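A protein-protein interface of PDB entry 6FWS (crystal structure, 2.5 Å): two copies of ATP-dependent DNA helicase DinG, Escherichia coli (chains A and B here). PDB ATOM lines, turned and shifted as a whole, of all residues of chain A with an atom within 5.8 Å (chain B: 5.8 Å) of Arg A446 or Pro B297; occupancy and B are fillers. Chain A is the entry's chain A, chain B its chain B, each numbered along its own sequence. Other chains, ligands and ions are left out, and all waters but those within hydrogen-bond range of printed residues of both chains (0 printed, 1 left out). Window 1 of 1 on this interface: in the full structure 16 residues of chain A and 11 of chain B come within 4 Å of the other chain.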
ATOM      1  N   ARG A 404       8.417 -10.697  -4.669  1.00  0.00           N
ATOM      2  CA  ARG A 404       7.815 -11.409  -3.551  1.00  0.00           C
ATOM      3  C   ARG A 404       8.734 -11.371  -2.336  1.00  0.00           C
ATOM      4  O   ARG A 404       8.263 -11.265  -1.200  1.00  0.00           O
ATOM      5  CB  ARG A 404       7.464 -12.840  -3.955  1.00  0.00           C
ATOM      6  CG  ARG A 404       6.121 -12.934  -4.692  1.00  0.00           C
ATOM      7  CD  ARG A 404       5.954 -14.216  -5.485  1.00  0.00           C
ATOM      8  NE  ARG A 404       6.636 -15.337  -4.859  1.00  0.00           N
ATOM      9  CZ  ARG A 404       7.606 -16.031  -5.439  1.00  0.00           C
ATOM     10  NH1 ARG A 404       7.999 -15.726  -6.668  1.00  0.00           N
ATOM     11  NH2 ARG A 404       8.175 -17.037  -4.793  1.00  0.00           N
ATOM     12  N   SER A 441      15.808 -20.979   7.186  1.00  0.00           N
ATOM     13  CA  SER A 441      15.392 -22.298   7.673  1.00  0.00           C
ATOM     14  C   SER A 441      14.115 -22.805   7.002  1.00  0.00           C
ATOM     15  O   SER A 441      14.044 -23.970   6.606  1.00  0.00           O
ATOM     16  CB  SER A 441      15.214 -22.261   9.196  1.00  0.00           C
ATOM     17  OG  SER A 441      14.201 -21.353   9.573  1.00  0.00           O
ATOM     18  N   ASP A 442      13.096 -21.950   6.865  1.00  0.00           N
ATOM     19  CA  ASP A 442      11.834 -22.392   6.267  1.00  0.00           C
ATOM     20  C   ASP A 442      12.005 -22.796   4.811  1.00  0.00           C
ATOM     21  O   ASP A 442      11.357 -23.747   4.346  1.00  0.00           O
ATOM     22  CB  ASP A 442      10.780 -21.297   6.390  1.00  0.00           C
ATOM     23  CG  ASP A 442      10.293 -21.131   7.805  1.00  0.00           C
ATOM     24  OD1 ASP A 442       9.131 -21.495   8.080  1.00  0.00           O
ATOM     25  OD2 ASP A 442      11.082 -20.663   8.654  1.00  0.00           O
ATOM     26  N   GLN A 443      12.882 -22.106   4.082  1.00  0.00           N
ATOM     27  CA  GLN A 443      13.140 -22.522   2.712  1.00  0.00           C
ATOM     28  C   GLN A 443      13.892 -23.839   2.670  1.00  0.00           C
ATOM     29  O   GLN A 443      13.632 -24.660   1.782  1.00  0.00           O
ATOM     30  CB  GLN A 443      13.895 -21.429   1.958  1.00  0.00           C
ATOM     31  CG  GLN A 443      13.105 -20.140   1.895  1.00  0.00           C
ATOM     32  CD  GLN A 443      13.519 -19.169   2.982  1.00  0.00           C
ATOM     33  OE1 GLN A 443      14.470 -18.407   2.805  1.00  0.00           O
ATOM     34  NE2 GLN A 443      12.814 -19.184   4.108  1.00  0.00           N
ATOM     35  N   LEU A 444      14.793 -24.079   3.632  1.00  0.00           N
ATOM     36  CA  LEU A 444      15.449 -25.383   3.709  1.00  0.00           C
ATOM     37  C   LEU A 444      14.430 -26.471   4.017  1.00  0.00           C
ATOM     38  O   LEU A 444      14.510 -27.584   3.477  1.00  0.00           O
ATOM     39  CB  LEU A 444      16.569 -25.356   4.754  1.00  0.00           C
ATOM     40  CG  LEU A 444      17.826 -24.554   4.362  1.00  0.00           C
ATOM     41  CD1 LEU A 444      18.839 -24.439   5.497  1.00  0.00           C
ATOM     42  CD2 LEU A 444      18.473 -25.186   3.175  1.00  0.00           C
ATOM     43  N   GLU A 445      13.444 -26.144   4.858  1.00  0.00           N
ATOM     44  CA  GLU A 445      12.326 -27.044   5.120  1.00  0.00           C
ATOM     45  C   GLU A 445      11.594 -27.411   3.840  1.00  0.00           C
ATOM     46  O   GLU A 445      11.231 -28.574   3.641  1.00  0.00           O
ATOM     47  CB  GLU A 445      11.352 -26.396   6.100  1.00  0.00           C
ATOM     48  CG  GLU A 445      10.250 -27.316   6.551  1.00  0.00           C
ATOM     49  CD  GLU A 445      10.751 -28.407   7.484  1.00  0.00           C
ATOM     50  OE1 GLU A 445      11.717 -28.148   8.240  1.00  0.00           O
ATOM     51  OE2 GLU A 445      10.184 -29.526   7.449  1.00  0.00           O
ATOM     52  N   ARG A 446      11.352 -26.436   2.963  1.00  0.00           N
ATOM     53  CA  ARG A 446      10.627 -26.761   1.738  1.00  0.00           C
ATOM     54  C   ARG A 446      11.501 -27.512   0.735  1.00  0.00           C
ATOM     55  O   ARG A 446      11.031 -28.451   0.085  1.00  0.00           O
ATOM     56  CB  ARG A 446      10.053 -25.494   1.102  1.00  0.00           C
ATOM     57  CG  ARG A 446       9.516 -25.713  -0.298  1.00  0.00           C
ATOM     58  CD  ARG A 446       8.757 -24.506  -0.812  1.00  0.00           C
ATOM     59  NE  ARG A 446       9.566 -23.286  -0.823  1.00  0.00           N
ATOM     60  CZ  ARG A 446      10.409 -22.958  -1.794  1.00  0.00           C
ATOM     61  NH1 ARG A 446      10.568 -23.768  -2.834  1.00  0.00           N
ATOM     62  NH2 ARG A 446      11.097 -21.826  -1.721  1.00  0.00           N
ATOM     63  N   LEU A 447      12.769 -27.127   0.597  1.00  0.00           N
ATOM     64  CA  LEU A 447      13.614 -27.656  -0.472  1.00  0.00           C
ATOM     65  C   LEU A 447      14.303 -28.962  -0.113  1.00  0.00           C
ATOM     66  O   LEU A 447      14.532 -29.799  -0.999  1.00  0.00           O
ATOM     67  CB  LEU A 447      14.683 -26.631  -0.858  1.00  0.00           C
ATOM     68  CG  LEU A 447      14.188 -25.386  -1.584  1.00  0.00           C
ATOM     69  CD1 LEU A 447      15.161 -24.238  -1.361  1.00  0.00           C
ATOM     70  CD2 LEU A 447      14.004 -25.678  -3.078  1.00  0.00           C
ATOM     71  N   LEU A 448      14.664 -29.147   1.157  1.00  0.00           N
ATOM     72  CA  LEU A 448      15.387 -30.346   1.570  1.00  0.00           C
ATOM     73  C   LEU A 448      14.636 -31.089   2.666  1.00  0.00           C
ATOM     74  O   LEU A 448      14.233 -32.231   2.449  1.00  0.00           O
ATOM     75  CB  LEU A 448      16.805 -29.986   2.021  1.00  0.00           C
ATOM     76  CG  LEU A 448      17.809 -29.502   0.973  1.00  0.00           C
ATOM     77  CD1 LEU A 448      19.089 -29.123   1.663  1.00  0.00           C
ATOM     78  CD2 LEU A 448      18.083 -30.581  -0.039  1.00  0.00           C
ATOM     79  N   TRP A 449      14.427 -30.479   3.833  1.00  0.00           N
ATOM     80  CA  TRP A 449      14.071 -31.248   5.018  1.00  0.00           C
ATOM     81  C   TRP A 449      12.823 -32.084   4.795  1.00  0.00           C
ATOM     82  O   TRP A 449      12.770 -33.258   5.184  1.00  0.00           O
ATOM     83  CB  TRP A 449      13.893 -30.313   6.207  1.00  0.00           C
ATOM     84  CG  TRP A 449      15.103 -29.472   6.508  1.00  0.00           C
ATOM     85  CD1 TRP A 449      15.096 -28.255   7.101  1.00  0.00           C
ATOM     86  CD2 TRP A 449      16.493 -29.780   6.235  1.00  0.00           C
ATOM     87  NE1 TRP A 449      16.372 -27.783   7.227  1.00  0.00           N
ATOM     88  CE2 TRP A 449      17.249 -28.694   6.704  1.00  0.00           C
ATOM     89  CE3 TRP A 449      17.165 -30.868   5.657  1.00  0.00           C
ATOM     90  CZ2 TRP A 449      18.642 -28.649   6.604  1.00  0.00           C
ATOM     91  CZ3 TRP A 449      18.548 -30.820   5.555  1.00  0.00           C
ATOM     92  CH2 TRP A 449      19.267 -29.720   6.033  1.00  0.00           C
ATOM     93  N   ARG A 450      11.821 -31.510   4.133  1.00  0.00           N
ATOM     94  CA  ARG A 450      10.560 -32.202   3.938  1.00  0.00           C
ATOM     95  C   ARG A 450      10.443 -32.871   2.569  1.00  0.00           C
ATOM     96  O   ARG A 450       9.558 -33.715   2.380  1.00  0.00           O
ATOM     97  CB  ARG A 450       9.409 -31.211   4.170  1.00  0.00           C
ATOM     98  CG  ARG A 450       8.269 -31.253   3.183  1.00  0.00           C
ATOM     99  CD  ARG A 450       7.139 -30.352   3.664  1.00  0.00           C
ATOM    100  NE  ARG A 450       7.506 -28.953   3.490  1.00  0.00           N
ATOM    101  CZ  ARG A 450       7.144 -27.976   4.315  1.00  0.00           C
ATOM    102  NH1 ARG A 450       6.401 -28.242   5.391  1.00  0.00           N
ATOM    103  NH2 ARG A 450       7.543 -26.731   4.066  1.00  0.00           N
ATOM    104  N   SER A 451      11.342 -32.554   1.634  1.00  0.00           N
ATOM    105  CA  SER A 451      11.337 -33.129   0.294  1.00  0.00           C
ATOM    106  C   SER A 451      12.099 -34.443   0.185  1.00  0.00           C
ATOM    107  O   SER A 451      11.684 -35.323  -0.580  1.00  0.00           O
ATOM    108  CB  SER A 451      11.933 -32.136  -0.706  1.00  0.00           C
ATOM    109  OG  SER A 451      11.959 -32.727  -1.989  1.00  0.00           O
ATOM    110  N   ILE B 295       4.789 -18.682   2.611  1.00  0.00           N
ATOM    111  CA  ILE B 295       3.881 -19.064   1.529  1.00  0.00           C
ATOM    112  C   ILE B 295       4.494 -20.204   0.732  1.00  0.00           C
ATOM    113  O   ILE B 295       5.630 -20.084   0.256  1.00  0.00           O
ATOM    114  CB  ILE B 295       3.576 -17.884   0.602  1.00  0.00           C
ATOM    115  CG1 ILE B 295       2.869 -16.783   1.383  1.00  0.00           C
ATOM    116  CG2 ILE B 295       2.732 -18.344  -0.562  1.00  0.00           C
ATOM    117  CD1 ILE B 295       2.551 -15.550   0.548  1.00  0.00           C
ATOM    118  N   PRO B 296       3.798 -21.317   0.557  1.00  0.00           N
ATOM    119  CA  PRO B 296       4.275 -22.338  -0.365  1.00  0.00           C
ATOM    120  C   PRO B 296       4.056 -21.873  -1.788  1.00  0.00           C
ATOM    121  O   PRO B 296       3.010 -21.279  -2.096  1.00  0.00           O
ATOM    122  CB  PRO B 296       3.401 -23.559  -0.042  1.00  0.00           C
ATOM    123  CG  PRO B 296       2.388 -23.109   0.973  1.00  0.00           C
ATOM    124  CD  PRO B 296       2.459 -21.624   1.084  1.00  0.00           C
ATOM    125  N   PRO B 297       5.023 -22.083  -2.675  1.00  0.00           N
ATOM    126  CA  PRO B 297       4.827 -21.641  -4.063  1.00  0.00           C
ATOM    127  C   PRO B 297       3.488 -22.070  -4.642  1.00  0.00           C
ATOM    128  O   PRO B 297       2.816 -21.250  -5.288  1.00  0.00           O
ATOM    129  CB  PRO B 297       6.009 -22.290  -4.798  1.00  0.00           C
ATOM    130  CG  PRO B 297       7.075 -22.368  -3.765  1.00  0.00           C
ATOM    131  CD  PRO B 297       6.369 -22.629  -2.450  1.00  0.00           C
ATOM    132  N   LEU B 298       3.062 -23.319  -4.401  1.00  0.00           N
ATOM    133  CA  LEU B 298       1.856 -23.805  -5.049  1.00  0.00           C
ATOM    134  C   LEU B 298       0.627 -23.068  -4.570  1.00  0.00           C
ATOM    135  O   LEU B 298      -0.431 -23.162  -5.193  1.00  0.00           O
ATOM    136  CB  LEU B 298       1.680 -25.305  -4.794  1.00  0.00           C
ATOM    137  CG  LEU B 298       0.619 -25.957  -5.672  1.00  0.00           C
ATOM    138  CD1 LEU B 298       0.982 -25.769  -7.122  1.00  0.00           C
ATOM    139  CD2 LEU B 298       0.493 -27.412  -5.334  1.00  0.00           C
ATOM    140  N   ALA B 299       0.741 -22.363  -3.455  1.00  0.00           N
ATOM    141  CA  ALA B 299      -0.428 -21.688  -2.933  1.00  0.00           C
ATOM    142  C   ALA B 299      -0.606 -20.318  -3.554  1.00  0.00           C
ATOM    143  O   ALA B 299      -1.650 -19.702  -3.335  1.00  0.00           O
ATOM    144  CB  ALA B 299      -0.371 -21.566  -1.407  1.00  0.00           C
ATOM    145  N   ILE B 300       0.342 -19.869  -4.367  1.00  0.00           N
ATOM    146  CA  ILE B 300       0.178 -18.628  -5.131  1.00  0.00           C
ATOM    147  C   ILE B 300      -0.941 -18.813  -6.151  1.00  0.00           C
ATOM    148  O   ILE B 300      -0.924 -19.795  -6.913  1.00  0.00           O
ATOM    149  CB  ILE B 300       1.493 -18.258  -5.814  1.00  0.00           C
ATOM    150  CG1 ILE B 300       2.580 -18.054  -4.760  1.00  0.00           C
ATOM    151  CG2 ILE B 300       1.328 -17.014  -6.697  1.00  0.00           C
ATOM    152  CD1 ILE B 300       3.962 -17.983  -5.323  1.00  0.00           C
ATOM    153  N   ARG B 303      -0.387 -19.887  -9.815  1.00  0.00           N
ATOM    154  CA  ARG B 303       0.178 -21.228  -9.909  1.00  0.00           C
ATOM    155  C   ARG B 303      -0.818 -22.298  -9.477  1.00  0.00           C
ATOM    156  O   ARG B 303      -0.912 -23.352 -10.115  1.00  0.00           O
ATOM    157  CB  ARG B 303       1.455 -21.314  -9.081  1.00  0.00           C
ATOM    158  CG  ARG B 303       2.590 -20.510  -9.681  1.00  0.00           C
ATOM    159  CD  ARG B 303       3.820 -20.494  -8.799  1.00  0.00           C
ATOM    160  NE  ARG B 303       4.686 -19.373  -9.153  1.00  0.00           N
ATOM    161  CZ  ARG B 303       5.845 -19.106  -8.563  1.00  0.00           C
ATOM    162  NH1 ARG B 303       6.281 -19.880  -7.578  1.00  0.00           N
ATOM    163  NH2 ARG B 303       6.557 -18.058  -8.953  1.00  0.00           N
ATOM    164  N   LEU B 304      -1.576 -22.059  -8.408  1.00  0.00           N
ATOM    165  CA  LEU B 304      -2.542 -23.071  -7.995  1.00  0.00           C
ATOM    166  C   LEU B 304      -3.621 -23.248  -9.054  1.00  0.00           C
ATOM    167  O   LEU B 304      -4.074 -24.372  -9.307  1.00  0.00           O
ATOM    168  CB  LEU B 304      -3.163 -22.706  -6.650  1.00  0.00           C
ATOM    169  CG  LEU B 304      -4.201 -23.703  -6.134  1.00  0.00           C
ATOM    170  CD1 LEU B 304      -3.591 -25.098  -5.990  1.00  0.00           C
ATOM    171  CD2 LEU B 304      -4.767 -23.213  -4.814  1.00  0.00           C
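Among the printed residues, pairs that only touch across the chains: Arg A404 with Ile B300 (3.8 Å), Arg A404 with Arg B303 (3.6 Å) and Arg A446 with Pro B297 (3.5 Å).
Hydrophobic or aromatic side chains of chain B that line the printed part of chain A: Pro B297 and Ile B300.
Of the 12 printed residues of chain A, 2 touch a printed residue of chain B.
Among the printed residues, 3 pairs touch across the chains.
Arg A446 touches just one residue of chain B: Pro B297.
Ile B295 touches none of the printed residues of chain A.
Printed residues of chain A within 4 Å of Pro B297: Arg A446 (3.5 Å).
Of the printed residues of chain A, Ile B300 touches Arg A404 (3.8 Å).
Of the printed residues of chain A, Arg B303 touches Arg A404 (3.6 Å).
The nearest residue of chain B that does not touch Arg A446 is Pro B296 (5.0 Å).
The nearest printed residue of chain A that does not touch Ile B300 is Arg A446 (8.9 Å).
No position is printed for both chains.
Of the 3 pairs that touch across the chains among the printed residues, none has its exchanged pair printed and touching as well.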
